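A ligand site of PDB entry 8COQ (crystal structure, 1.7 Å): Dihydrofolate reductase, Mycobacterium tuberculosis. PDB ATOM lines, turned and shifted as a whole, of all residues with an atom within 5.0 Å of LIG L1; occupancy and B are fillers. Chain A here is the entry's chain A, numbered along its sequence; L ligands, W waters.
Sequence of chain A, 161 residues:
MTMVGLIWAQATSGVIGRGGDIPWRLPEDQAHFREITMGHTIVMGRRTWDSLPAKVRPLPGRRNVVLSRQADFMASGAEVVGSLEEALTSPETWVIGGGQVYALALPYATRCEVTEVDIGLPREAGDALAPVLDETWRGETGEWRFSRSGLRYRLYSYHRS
The backbone carbonyl oxygen (O) of Ala 9 lies close to an oxygen (O14) of LIG L1 (2.8 Å). O of Ile 16 sits close to O14 of LIG L1 (3.1 Å). Merely in contact with LIG L1: Leu 67 (3.3 Å), Ile 96 (3.3 Å), Gly 17 (3.3 Å), Trp 8 (3.4 Å), Gly 82 (3.4 Å), Gly 20 (3.5 Å), Gly 45 (3.5 Å), Leu 104 (3.6 Å), Arg 18 (3.6 Å), Ile 22 (3.6 Å), Tyr 102 (3.7 Å), Gly 97 (3.9 Å) and Ala 128 (3.96 Å). Hydrophobic or aromatic side chains that line LIG L1: Trp 8, Ile 16, Ile 22, Leu 67, Val 101, Leu 104 and Ala 128. Within 4 Å of LIG L1: Trp 8, Ala 9, Ile 16, Gly 17, Arg 18, Gly 20, Asp 21, Ile 22, Gly 45, Arg 46, Arg 47, Thr 48, Leu 67, Ser 68, Arg 69, Gln 70, Gly 82, Ile 96, Gly 97, Gly 98, Gly 99, Gln 100, Val 101, Tyr 102, Leu 104 and Ala 128.
Water W5 lies within hydrogen-bond range of O16 of LIG L1 and NH1 of Arg 69. Water W2 lies within hydrogen-bond range of O13 of LIG L1 (2.7 Å) and OG of Ser 51 (2.8 Å). Water W4 lies within hydrogen-bond range of N of Gly 20 (2.9 Å), O12 of LIG L1 (3.0 Å) and N of Arg 18 (3.3 Å).
O2 of LIG L1 is in hydrogen-bond range of OG1 of Thr 48 (2.7 Å). An oxygen (O1) of LIG L1 is in hydrogen-bond range of the backbone NH (N) of Val 101, 3.4 Å away. The backbone NH of Asp 21 sits at hydrogen-bond distance from an oxygen (O12) of LIG L1, 3.4 Å away. The backbone NH (N) of Arg 69 lies within hydrogen-bond range of an oxygen (O16) of LIG L1, 2.9 Å away. The side-chain hydroxyl (OG) of Ser 68 lies within hydrogen-bond range of an oxygen (O15) of LIG L1 (2.8 Å). The backbone NH (N) of Arg 47 is in hydrogen-bond range of an oxygen (O3) of LIG L1, 3.5 Å away. The backbone NH of Gly 99 is in hydrogen-bond range of an oxygen (O8) of LIG L1. The backbone NH (N) of Gly 98 sits at hydrogen-bond distance from an oxygen (O2) of LIG L1, at 2.9 Å. The side-chain hydroxyl (OH) of Tyr 102 is in hydrogen-bond range of a nitrogen (N3) of LG2 L2, at 3.4 Å. The side-chain amide oxygen of Gln 70 lies close to an oxygen (O15) of LIG L1 (3.3 Å). The backbone carbonyl oxygen (O) of Asp 21 sits at hydrogen-bond distance from an oxygen (O12) of LIG L1. O of Ile 96 sits at hydrogen-bond distance from N3 of LG2 L2 (2.9 Å). The backbone NH of Gln 100 lies within hydrogen-bond range of an oxygen (O8) of LIG L1 (3.0 Å). The guanidinium group (NH1) of Arg 47 lies within salt-bridge range of an oxygen (O9) of LIG L1 (3.1 Å). The backbone carbonyl oxygen (O) of Ile 7 is in hydrogen-bond range of a nitrogen (N3) of LG2 L2 (3.0 Å). The guanidinium group of Arg 46 is in salt-bridge range of an oxygen (O15) of LIG L1 (2.8 Å). An oxygen (O4) of LIG L1 is in hydrogen-bond range of the backbone NH of Arg 46. The backbone NH of Thr 48 is in hydrogen-bond range of an oxygen (O2) of LIG L1, 3.2 Å away.
N of Gly 45 lies within hydrogen-bond range of O of Gly 97. N of Ile 16 lies within hydrogen-bond range of O of Ala 128 (2.8 Å). The side-chain hydroxyl of Ser 68 is in hydrogen-bond range of the backbone NH of Gln 70 (3.0 Å). O of Leu 67 is in hydrogen-bond range of N of Arg 46. The side-chain hydroxyl (OG1) of Thr 48 is in hydrogen-bond range of the backbone NH (N) of Gly 98, 3.1 Å away. The backbone carbonyl oxygen (O) of Gly 17 is in hydrogen-bond range of the backbone NH (N) of Ala 128, at 3.0 Å. N of Gly 97 sits close to OH of Tyr 102, at 3.5 Å. OH of Tyr 102 lies within hydrogen-bond range of O of Ile 7 (2.6 Å).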
ATOM      1  N   ILE A   7     -16.920  14.823  16.689  1.00  0.00           N
ATOM      2  CA  ILE A   7     -16.991  15.487  15.389  1.00  0.00           C
ATOM      3  C   ILE A   7     -15.647  15.299  14.689  1.00  0.00           C
ATOM      4  O   ILE A   7     -14.602  15.455  15.323  1.00  0.00           O
ATOM      5  CB  ILE A   7     -17.395  16.975  15.528  1.00  0.00           C
ATOM      6  CG1 ILE A   7     -17.478  17.666  14.155  1.00  0.00           C
ATOM      7  CG2 ILE A   7     -16.482  17.718  16.477  1.00  0.00           C
ATOM      8  CD1 ILE A   7     -18.141  19.056  14.230  1.00  0.00           C
ATOM      9  N   TRP A   8     -15.689  14.888  13.414  1.00  0.00           N
ATOM     10  CA  TRP A   8     -14.455  14.681  12.653  1.00  0.00           C
ATOM     11  C   TRP A   8     -14.736  14.804  11.165  1.00  0.00           C
ATOM     12  O   TRP A   8     -15.880  14.686  10.705  1.00  0.00           O
ATOM     13  CB  TRP A   8     -13.809  13.303  12.962  1.00  0.00           C
ATOM     14  CG  TRP A   8     -14.478  12.076  12.378  1.00  0.00           C
ATOM     15  CD1 TRP A   8     -14.388  11.617  11.099  1.00  0.00           C
ATOM     16  CD2 TRP A   8     -15.355  11.158  13.068  1.00  0.00           C
ATOM     17  NE1 TRP A   8     -15.110  10.465  10.945  1.00  0.00           N
ATOM     18  CE2 TRP A   8     -15.730  10.170  12.139  1.00  0.00           C
ATOM     19  CE3 TRP A   8     -15.843  11.084  14.372  1.00  0.00           C
ATOM     20  CZ2 TRP A   8     -16.564   9.105  12.470  1.00  0.00           C
ATOM     21  CZ3 TRP A   8     -16.683  10.005  14.705  1.00  0.00           C
ATOM     22  CH2 TRP A   8     -17.045   9.048  13.751  1.00  0.00           C
ATOM     23  N   ALA A   9     -13.658  15.011  10.409  1.00  0.00           N
ATOM     24  CA  ALA A   9     -13.671  14.971   8.954  1.00  0.00           C
ATOM     25  C   ALA A   9     -12.793  13.821   8.483  1.00  0.00           C
ATOM     26  O   ALA A   9     -11.673  13.654   8.972  1.00  0.00           O
ATOM     27  CB  ALA A   9     -13.148  16.283   8.358  1.00  0.00           C
ATOM     28  N   ILE A  16      -8.136  10.232   8.807  1.00  0.00           N
ATOM     29  CA  ILE A  16      -8.426  11.542   9.376  1.00  0.00           C
ATOM     30  C   ILE A  16      -7.179  12.349   9.638  1.00  0.00           C
ATOM     31  O   ILE A  16      -7.278  13.568   9.846  1.00  0.00           O
ATOM     32  CB  ILE A  16      -9.264  11.435  10.660  1.00  0.00           C
ATOM     33  CG1 ILE A  16      -8.438  10.782  11.775  1.00  0.00           C
ATOM     34  CG2 ILE A  16     -10.592  10.644  10.409  1.00  0.00           C
ATOM     35  CD1 ILE A  16      -8.872  11.189  13.163  1.00  0.00           C
ATOM     36  N   GLY A  17      -6.002  11.750   9.632  1.00  0.00           N
ATOM     37  CA  GLY A  17      -4.805  12.498   9.926  1.00  0.00           C
ATOM     38  C   GLY A  17      -3.597  11.786   9.365  1.00  0.00           C
ATOM     39  O   GLY A  17      -3.579  10.555   9.251  1.00  0.00           O
ATOM     40  N   ARG A  18      -2.588  12.568   9.014  1.00  0.00           N
ATOM     41  CA  ARG A  18      -1.370  12.016   8.444  1.00  0.00           C
ATOM     42  C   ARG A  18      -0.213  12.958   8.750  1.00  0.00           C
ATOM     43  O   ARG A  18      -0.319  14.164   8.489  1.00  0.00           O
ATOM     44  CB  ARG A  18      -1.531  11.811   6.937  1.00  0.00           C
ATOM     45  CG  ARG A  18      -0.318  11.255   6.262  1.00  0.00           C
ATOM     46  CD  ARG A  18      -0.652  10.937   4.822  1.00  0.00           C
ATOM     47  NE  ARG A  18      -1.473   9.737   4.730  1.00  0.00           N
ATOM     48  CZ  ARG A  18      -1.974   9.263   3.596  1.00  0.00           C
ATOM     49  NH1 ARG A  18      -1.747   9.916   2.446  1.00  0.00           N
ATOM     50  NH2 ARG A  18      -2.711   8.163   3.602  1.00  0.00           N
ATOM     51  N   GLY A  20       0.823  14.115  11.459  1.00  0.00           N
ATOM     52  CA  GLY A  20       0.525  15.127  12.485  1.00  0.00           C
ATOM     53  C   GLY A  20      -0.320  16.263  11.965  1.00  0.00           C
ATOM     54  O   GLY A  20      -0.530  17.199  12.671  1.00  0.00           O
ATOM     55  N   ASP A  21      -0.801  16.161  10.735  1.00  0.00           N
ATOM     56  CA  ASP A  21      -1.689  17.186  10.172  1.00  0.00           C
ATOM     57  C   ASP A  21      -2.856  16.505   9.428  1.00  0.00           C
ATOM     58  O   ASP A  21      -3.143  15.355   9.719  1.00  0.00           O
ATOM     59  CB  ASP A  21      -0.931  18.257   9.376  1.00  0.00           C
ATOM     60  CG  ASP A  21      -1.562  19.622   9.444  1.00  0.00           C
ATOM     61  OD1 ASP A  21      -2.465  19.864   8.696  1.00  0.00           O
ATOM     62  OD2 ASP A  21      -1.181  20.352  10.241  1.00  0.00           O
ATOM     63  N   ILE A  22      -3.465  17.229   8.496  1.00  0.00           N
ATOM     64  CA  ILE A  22      -4.631  16.784   7.693  1.00  0.00           C
ATOM     65  C   ILE A  22      -4.343  17.050   6.221  1.00  0.00           C
ATOM     66  O   ILE A  22      -3.935  18.106   5.901  1.00  0.00           O
ATOM     67  CB  ILE A  22      -5.876  17.491   8.200  1.00  0.00           C
ATOM     68  CG1 ILE A  22      -6.180  17.077   9.624  1.00  0.00           C
ATOM     69  CG2 ILE A  22      -7.047  17.179   7.312  1.00  0.00           C
ATOM     70  CD1 ILE A  22      -6.933  18.107  10.340  1.00  0.00           C
ATOM     71  N   TRP A  24      -5.916  17.873   3.555  1.00  0.00           N
ATOM     72  CA  TRP A  24      -6.922  18.639   2.820  1.00  0.00           C
ATOM     73  C   TRP A  24      -7.263  19.847   3.680  1.00  0.00           C
ATOM     74  O   TRP A  24      -6.861  19.928   4.832  1.00  0.00           O
ATOM     75  CB  TRP A  24      -8.181  17.809   2.524  1.00  0.00           C
ATOM     76  CG  TRP A  24      -8.948  17.435   3.780  1.00  0.00           C
ATOM     77  CD1 TRP A  24      -9.770  18.224   4.517  1.00  0.00           C
ATOM     78  CD2 TRP A  24      -8.942  16.160   4.404  1.00  0.00           C
ATOM     79  NE1 TRP A  24     -10.281  17.515   5.587  1.00  0.00           N
ATOM     80  CE2 TRP A  24      -9.784  16.239   5.541  1.00  0.00           C
ATOM     81  CE3 TRP A  24      -8.314  14.940   4.122  1.00  0.00           C
ATOM     82  CZ2 TRP A  24     -10.001  15.161   6.377  1.00  0.00           C
ATOM     83  CZ3 TRP A  24      -8.516  13.870   4.955  1.00  0.00           C
ATOM     84  CH2 TRP A  24      -9.361  13.988   6.068  1.00  0.00           C
ATOM     85  N   GLY A  45      -6.949  15.246  22.060  1.00  0.00           N
ATOM     86  CA  GLY A  45      -5.733  14.588  22.519  1.00  0.00           C
ATOM     87  C   GLY A  45      -4.552  15.527  22.474  1.00  0.00           C
ATOM     88  O   GLY A  45      -4.579  16.552  21.791  1.00  0.00           O
ATOM     89  N   ARG A  46      -3.488  15.184  23.214  1.00  0.00           N
ATOM     90  CA  ARG A  46      -2.335  16.083  23.296  1.00  0.00           C
ATOM     91  C   ARG A  46      -1.692  16.297  21.938  1.00  0.00           C
ATOM     92  O   ARG A  46      -1.258  17.405  21.625  1.00  0.00           O
ATOM     93  CB  ARG A  46      -1.306  15.537  24.286  1.00  0.00           C
ATOM     94  CG  ARG A  46      -0.262  16.584  24.682  1.00  0.00           C
ATOM     95  CD  ARG A  46       1.055  16.413  23.896  1.00  0.00           C
ATOM     96  NE  ARG A  46       1.553  15.040  23.945  1.00  0.00           N
ATOM     97  CZ  ARG A  46       2.279  14.480  22.985  1.00  0.00           C
ATOM     98  NH1 ARG A  46       2.617  15.175  21.901  1.00  0.00           N
ATOM     99  NH2 ARG A  46       2.692  13.227  23.107  1.00  0.00           N
ATOM    100  N   ARG A  47      -1.640  15.246  21.112  1.00  0.00           N
ATOM    101  CA  ARG A  47      -1.074  15.390  19.780  1.00  0.00           C
ATOM    102  C   ARG A  47      -1.865  16.379  18.943  1.00  0.00           C
ATOM    103  O   ARG A  47      -1.296  17.148  18.162  1.00  0.00           O
ATOM    104  CB  ARG A  47      -1.011  14.030  19.091  1.00  0.00           C
ATOM    105  CG  ARG A  47       0.095  13.118  19.562  1.00  0.00           C
ATOM    106  CD  ARG A  47       0.115  11.887  18.685  1.00  0.00           C
ATOM    107  NE  ARG A  47       0.991  10.839  19.202  1.00  0.00           N
ATOM    108  CZ  ARG A  47       0.976   9.581  18.765  1.00  0.00           C
ATOM    109  NH1 ARG A  47       0.112   9.218  17.824  1.00  0.00           N
ATOM    110  NH2 ARG A  47       1.816   8.691  19.282  1.00  0.00           N
ATOM    111  N   THR A  48      -3.197  16.369  19.085  1.00  0.00           N
ATOM    112  CA  THR A  48      -4.003  17.321  18.331  1.00  0.00           C
ATOM    113  C   THR A  48      -3.790  18.758  18.807  1.00  0.00           C
ATOM    114  O   THR A  48      -3.734  19.687  17.991  1.00  0.00           O
ATOM    115  CB  THR A  48      -5.473  16.913  18.373  1.00  0.00           C
ATOM    116  OG1 THR A  48      -5.613  15.689  17.628  1.00  0.00           O
ATOM    117  CG2 THR A  48      -6.415  18.013  17.771  1.00  0.00           C
ATOM    118  N   SER A  51      -0.833  20.088  17.267  1.00  0.00           N
ATOM    119  CA  SER A  51      -1.007  20.383  15.847  1.00  0.00           C
ATOM    120  C   SER A  51      -1.514  21.791  15.617  1.00  0.00           C
ATOM    121  O   SER A  51      -1.343  22.326  14.504  1.00  0.00           O
ATOM    122  CB  SER A  51      -1.939  19.351  15.206  1.00  0.00           C
ATOM    123  OG  SER A  51      -3.299  19.672  15.424  1.00  0.00           O
ATOM    124  N   LEU A  67      -6.265  16.139  26.730  1.00  0.00           N
ATOM    125  CA  LEU A  67      -6.028  14.861  27.388  1.00  0.00           C
ATOM    126  C   LEU A  67      -4.545  14.491  27.236  1.00  0.00           C
ATOM    127  O   LEU A  67      -4.035  14.390  26.118  1.00  0.00           O
ATOM    128  CB  LEU A  67      -6.949  13.801  26.805  1.00  0.00           C
ATOM    129  CG  LEU A  67      -7.087  12.394  27.354  1.00  0.00           C
ATOM    130  CD1 LEU A  67      -7.466  12.377  28.823  1.00  0.00           C
ATOM    131  CD2 LEU A  67      -8.207  11.768  26.537  1.00  0.00           C
ATOM    132  N   SER A  68      -3.865  14.296  28.367  1.00  0.00           N
ATOM    133  CA  SER A  68      -2.454  13.955  28.353  1.00  0.00           C
ATOM    134  C   SER A  68      -2.163  13.105  29.577  1.00  0.00           C
ATOM    135  O   SER A  68      -2.771  13.306  30.621  1.00  0.00           O
ATOM    136  CB  SER A  68      -1.551  15.192  28.371  1.00  0.00           C
ATOM    137  OG  SER A  68      -0.170  14.833  28.411  1.00  0.00           O
ATOM    138  N   ARG A  69      -1.244  12.160  29.432  1.00  0.00           N
ATOM    139  CA  ARG A  69      -0.756  11.403  30.568  1.00  0.00           C
ATOM    140  C   ARG A  69       0.441  12.082  31.232  1.00  0.00           C
ATOM    141  O   ARG A  69       0.963  11.566  32.234  1.00  0.00           O
ATOM    142  CB  ARG A  69      -0.363  10.003  30.107  1.00  0.00           C
ATOM    143  CG  ARG A  69      -1.554   9.084  29.795  1.00  0.00           C
ATOM    144  CD  ARG A  69      -1.044   7.690  29.439  1.00  0.00           C
ATOM    145  NE  ARG A  69      -2.065   6.817  28.846  1.00  0.00           N
ATOM    146  CZ  ARG A  69      -2.276   6.703  27.540  1.00  0.00           C
ATOM    147  NH1 ARG A  69      -1.546   7.418  26.696  1.00  0.00           N
ATOM    148  NH2 ARG A  69      -3.209   5.893  27.069  1.00  0.00           N
ATOM    149  N   GLN A  70       0.889  13.211  30.709  1.00  0.00           N
ATOM    150  CA  GLN A  70       2.001  13.949  31.273  1.00  0.00           C
ATOM    151  C   GLN A  70       1.480  14.887  32.366  1.00  0.00           C
ATOM    152  O   GLN A  70       0.820  15.887  32.074  1.00  0.00           O
ATOM    153  CB  GLN A  70       2.744  14.728  30.187  1.00  0.00           C
ATOM    154  CG  GLN A  70       3.486  13.832  29.195  1.00  0.00           C
ATOM    155  CD  GLN A  70       4.206  14.606  28.110  1.00  0.00           C
ATOM    156  OE1 GLN A  70       3.648  14.892  27.033  1.00  0.00           O
ATOM    157  NE2 GLN A  70       5.461  14.968  28.373  1.00  0.00           N
ATOM    158  N   GLY A  82      -6.066  14.105  32.908  1.00  0.00           N
ATOM    159  CA  GLY A  82      -5.428  12.804  32.762  1.00  0.00           C
ATOM    160  C   GLY A  82      -6.384  11.708  32.371  1.00  0.00           C
ATOM    161  O   GLY A  82      -5.953  10.615  31.977  1.00  0.00           O
ATOM    162  N   SER A  83      -7.682  11.980  32.447  1.00  0.00           N
ATOM    163  CA  SER A  83      -8.693  11.003  32.049  1.00  0.00           C
ATOM    164  C   SER A  83      -9.820  11.746  31.360  1.00  0.00           C
ATOM    165  O   SER A  83     -10.019  12.939  31.556  1.00  0.00           O
ATOM    166  CB  SER A  83      -9.243  10.227  33.249  1.00  0.00           C
ATOM    167  OG  SER A  83      -9.691  11.112  34.263  1.00  0.00           O
ATOM    168  N   ILE A  96     -13.029  16.388  19.731  1.00  0.00           N
ATOM    169  CA  ILE A  96     -12.624  16.936  18.436  1.00  0.00           C
ATOM    170  C   ILE A  96     -11.369  16.274  17.888  1.00  0.00           C
ATOM    171  O   ILE A  96     -10.800  16.755  16.901  1.00  0.00           O
ATOM    172  CB  ILE A  96     -12.436  18.462  18.484  1.00  0.00           C
ATOM    173  CG1 ILE A  96     -11.224  18.837  19.341  1.00  0.00           C
ATOM    174  CG2 ILE A  96     -13.659  19.095  19.047  1.00  0.00           C
ATOM    175  CD1 ILE A  96     -10.927  20.363  19.310  1.00  0.00           C
ATOM    176  N   GLY A  97     -10.926  15.174  18.485  1.00  0.00           N
ATOM    177  CA  GLY A  97      -9.837  14.377  17.927  1.00  0.00           C
ATOM    178  C   GLY A  97      -8.636  14.332  18.848  1.00  0.00           C
ATOM    179  O   GLY A  97      -8.589  14.999  19.875  1.00  0.00           O
ATOM    180  N   GLY A  98      -7.647  13.525  18.455  1.00  0.00           N
ATOM    181  CA  GLY A  98      -7.645  12.811  17.194  1.00  0.00           C
ATOM    182  C   GLY A  98      -8.043  11.349  17.289  1.00  0.00           C
ATOM    183  O   GLY A  98      -8.971  10.991  18.035  1.00  0.00           O
ATOM    184  N   GLY A  99      -7.329  10.494  16.559  1.00  0.00           N
ATOM    185  CA  GLY A  99      -7.760   9.116  16.399  1.00  0.00           C
ATOM    186  C   GLY A  99      -7.835   8.332  17.694  1.00  0.00           C
ATOM    187  O   GLY A  99      -8.761   7.544  17.890  1.00  0.00           O
ATOM    188  N   GLN A 100      -6.855   8.522  18.586  1.00  0.00           N
ATOM    189  CA  GLN A 100      -6.864   7.806  19.861  1.00  0.00           C
ATOM    190  C   GLN A 100      -7.993   8.273  20.754  1.00  0.00           C
ATOM    191  O   GLN A 100      -8.647   7.448  21.404  1.00  0.00           O
ATOM    192  CB  GLN A 100      -5.517   7.964  20.580  1.00  0.00           C
ATOM    193  CG  GLN A 100      -4.320   7.377  19.851  1.00  0.00           C
ATOM    194  CD  GLN A 100      -3.026   7.559  20.621  1.00  0.00           C
ATOM    195  OE1 GLN A 100      -3.054   7.921  21.813  1.00  0.00           O
ATOM    196  NE2 GLN A 100      -1.898   7.262  19.990  1.00  0.00           N
ATOM    197  N   VAL A 101      -8.228   9.584  20.819  1.00  0.00           N
ATOM    198  CA  VAL A 101      -9.288  10.078  21.689  1.00  0.00           C
ATOM    199  C   VAL A 101     -10.673   9.717  21.144  1.00  0.00           C
ATOM    200  O   VAL A 101     -11.607   9.460  21.922  1.00  0.00           O
ATOM    201  CB  VAL A 101      -9.114  11.588  21.926  1.00  0.00           C
ATOM    202  CG1 VAL A 101     -10.232  12.145  22.823  1.00  0.00           C
ATOM    203  CG2 VAL A 101      -7.753  11.847  22.555  1.00  0.00           C
ATOM    204  N   TYR A 102     -10.861   9.723  19.817  1.00  0.00           N
ATOM    205  CA  TYR A 102     -12.124   9.246  19.253  1.00  0.00           C
ATOM    206  C   TYR A 102     -12.429   7.841  19.749  1.00  0.00           C
ATOM    207  O   TYR A 102     -13.531   7.572  20.249  1.00  0.00           O
ATOM    208  CB  TYR A 102     -12.069   9.260  17.730  1.00  0.00           C
ATOM    209  CG  TYR A 102     -12.123  10.640  17.127  1.00  0.00           C
ATOM    210  CD1 TYR A 102     -11.337  10.954  16.026  1.00  0.00           C
ATOM    211  CD2 TYR A 102     -12.967  11.629  17.633  1.00  0.00           C
ATOM    212  CE1 TYR A 102     -11.362  12.207  15.455  1.00  0.00           C
ATOM    213  CE2 TYR A 102     -13.005  12.903  17.060  1.00  0.00           C
ATOM    214  CZ  TYR A 102     -12.198  13.168  15.956  1.00  0.00           C
ATOM    215  OH  TYR A 102     -12.177  14.403  15.362  1.00  0.00           O
ATOM    216  N   LEU A 104     -11.284   6.311  22.395  1.00  0.00           N
ATOM    217  CA  LEU A 104     -11.486   6.318  23.849  1.00  0.00           C
ATOM    218  C   LEU A 104     -12.837   6.902  24.247  1.00  0.00           C
ATOM    219  O   LEU A 104     -13.410   6.483  25.264  1.00  0.00           O
ATOM    220  CB  LEU A 104     -10.343   7.092  24.500  1.00  0.00           C
ATOM    221  CG  LEU A 104     -10.326   7.441  25.989  1.00  0.00           C
ATOM    222  CD1 LEU A 104      -9.951   6.255  26.819  1.00  0.00           C
ATOM    223  CD2 LEU A 104      -9.307   8.539  26.197  1.00  0.00           C
ATOM    224  N   ALA A 128      -3.854   8.295  11.240  1.00  0.00           N
ATOM    225  CA  ALA A 128      -4.916   8.269  12.219  1.00  0.00           C
ATOM    226  C   ALA A 128      -6.240   8.022  11.508  1.00  0.00           C
ATOM    227  O   ALA A 128      -6.484   8.568  10.424  1.00  0.00           O
ATOM    228  CB  ALA A 128      -4.932   9.607  12.971  1.00  0.00           C
HETATM  229  P1  LIG L   1      -4.444  12.277  19.554  1.00  0.00           P
HETATM  230  O1  LIG L   1      -5.538  11.351  19.712  1.00  0.00           O
HETATM  231  O2  LIG L   1      -4.786  13.603  19.113  1.00  0.00           O
HETATM  232  O3  LIG L   1      -3.587  12.375  20.849  1.00  0.00           O
HETATM  233  C1  LIG L   1      -3.071  11.195  21.462  1.00  0.00           C
HETATM  234  C2  LIG L   1      -2.459  11.564  22.798  1.00  0.00           C
HETATM  235  O4  LIG L   1      -3.511  11.842  23.731  1.00  0.00           O
HETATM  236  C3  LIG L   1      -1.590  10.538  23.519  1.00  0.00           C
HETATM  237  O5  LIG L   1      -0.264  10.714  23.062  1.00  0.00           O
HETATM  238  C4  LIG L   1      -1.696  11.025  24.953  1.00  0.00           C
HETATM  239  O6  LIG L   1      -0.976  12.193  25.155  1.00  0.00           O
HETATM  240  C5  LIG L   1      -3.167  11.400  25.011  1.00  0.00           C
HETATM  241  N1  LIG L   1      -4.012  10.285  25.404  1.00  0.00           N
HETATM  242  C6  LIG L   1      -4.457   9.282  24.632  1.00  0.00           C
HETATM  243  N2  LIG L   1      -5.173   8.398  25.271  1.00  0.00           N
HETATM  244  C7  LIG L   1      -5.159   8.842  26.572  1.00  0.00           C
HETATM  245  C8  LIG L   1      -5.733   8.342  27.747  1.00  0.00           C
HETATM  246  N3  LIG L   1      -6.424   7.221  27.817  1.00  0.00           N
HETATM  247  N4  LIG L   1      -5.518   9.031  28.882  1.00  0.00           N
HETATM  248  C9  LIG L   1      -4.827  10.154  28.826  1.00  0.00           C
HETATM  249  N5  LIG L   1      -4.261  10.722  27.774  1.00  0.00           N
HETATM  250  C10 LIG L   1      -4.453  10.010  26.668  1.00  0.00           C
HETATM  251  O7  LIG L   1      -3.417  11.653  18.542  1.00  0.00           O
HETATM  252  P2  LIG L   1      -3.605  10.920  17.168  1.00  0.00           P
HETATM  253  O8  LIG L   1      -4.449   9.775  17.287  1.00  0.00           O
HETATM  254  O9  LIG L   1      -2.297  10.672  16.604  1.00  0.00           O
HETATM  255  O10 LIG L   1      -4.352  11.958  16.265  1.00  0.00           O
HETATM  256  C11 LIG L   1      -3.662  13.078  15.776  1.00  0.00           C
HETATM  257  C12 LIG L   1      -3.955  13.242  14.313  1.00  0.00           C
HETATM  258  O11 LIG L   1      -5.366  13.390  14.061  1.00  0.00           O
HETATM  259  C13 LIG L   1      -3.283  14.430  13.612  1.00  0.00           C
HETATM  260  O12 LIG L   1      -3.009  14.080  12.265  1.00  0.00           O
HETATM  261  C14 LIG L   1      -4.421  15.414  13.563  1.00  0.00           C
HETATM  262  O13 LIG L   1      -4.193  16.407  12.607  1.00  0.00           O
HETATM  263  C15 LIG L   1      -5.557  14.476  13.191  1.00  0.00           C
HETATM  264  N6  LIG L   1      -6.865  15.089  13.419  1.00  0.00           N
HETATM  265  C16 LIG L   1      -7.856  15.040  12.486  1.00  0.00           C
HETATM  266  C17 LIG L   1      -9.069  15.574  12.701  1.00  0.00           C
HETATM  267  C18 LIG L   1     -10.122  15.471  11.670  1.00  0.00           C
HETATM  268  O14 LIG L   1      -9.845  15.116  10.538  1.00  0.00           O
HETATM  269  N7  LIG L   1     -11.347  15.790  12.007  1.00  0.00           N
HETATM  270  C19 LIG L   1      -9.290  16.272  13.945  1.00  0.00           C
HETATM  271  C20 LIG L   1      -8.217  16.214  14.904  1.00  0.00           C
HETATM  272  C21 LIG L   1      -7.082  15.682  14.602  1.00  0.00           C
HETATM  273  P3  LIG L   1       0.427  12.165  25.859  1.00  0.00           P
HETATM  274  O15 LIG L   1       0.742  13.527  26.136  1.00  0.00           O
HETATM  275  O16 LIG L   1       0.208  11.366  27.009  1.00  0.00           O
HETATM  276  O17 LIG L   1       1.338  11.573  24.910  1.00  0.00           O
HETATM  277  C1  LG2 L   2      -9.503  21.331   9.933  1.00  0.00           C
HETATM  278  C2  LG2 L   2     -11.233  22.214  11.975  1.00  0.00           C
HETATM  279  C3  LG2 L   2      -7.605  20.927  15.226  1.00  0.00           C
HETATM  280  C4  LG2 L   2     -14.260  18.524  11.723  1.00  0.00           C
HETATM  281  C5  LG2 L   2     -12.266  19.847  12.008  1.00  0.00           C
HETATM  282  C6  LG2 L   2     -12.011  19.248  13.210  1.00  0.00           C
HETATM  283  C7  LG2 L   2     -12.962  18.306  13.580  1.00  0.00           C
HETATM  284  C8  LG2 L   2     -10.817  19.560  14.117  1.00  0.00           C
HETATM  285  C9  LG2 L   2      -9.910  19.793  14.839  1.00  0.00           C
HETATM  286  C10 LG2 L   2      -8.739  20.057  15.781  1.00  0.00           C
HETATM  287  C11 LG2 L   2     -11.295  20.909  11.489  1.00  0.00           C
HETATM  288  C12 LG2 L   2     -10.446  20.466  10.487  1.00  0.00           C
HETATM  289  C13 LG2 L   2      -9.446  22.630  10.413  1.00  0.00           C
HETATM  290  C14 LG2 L   2     -10.290  23.080  11.421  1.00  0.00           C
HETATM  291  C15 LG2 L   2      -9.848  18.623   9.036  1.00  0.00           C
HETATM  292  C16 LG2 L   2      -8.637  21.519  16.227  1.00  0.00           C
HETATM  293  N1  LG2 L   2     -14.036  17.952  12.896  1.00  0.00           N
HETATM  294  N2  LG2 L   2     -13.333  19.438  11.351  1.00  0.00           N
HETATM  295  N3  LG2 L   2     -12.707  17.679  14.863  1.00  0.00           N
HETATM  296  N4  LG2 L   2     -15.413  18.201  10.872  1.00  0.00           N
HETATM  297  O1  LG2 L   2     -10.639  19.112  10.115  1.00  0.00           O
HETATM  298  O   HOH W   1      -0.657  11.581  14.370  1.00  0.00           O
HETATM  299  O   HOH W   2      -5.013  18.823  13.369  1.00  0.00           O
HETATM  300  O   HOH W   3      -6.038   5.772  24.612  1.00  0.00           O
HETATM  301  O   HOH W   4      -1.008  11.939  11.795  1.00  0.00           O
HETATM  302  O   HOH W   5       0.836   8.843  26.821  1.00  0.00           O
HETATM  303  O   HOH W   6      -3.872   7.514  15.872  1.00  0.00           O
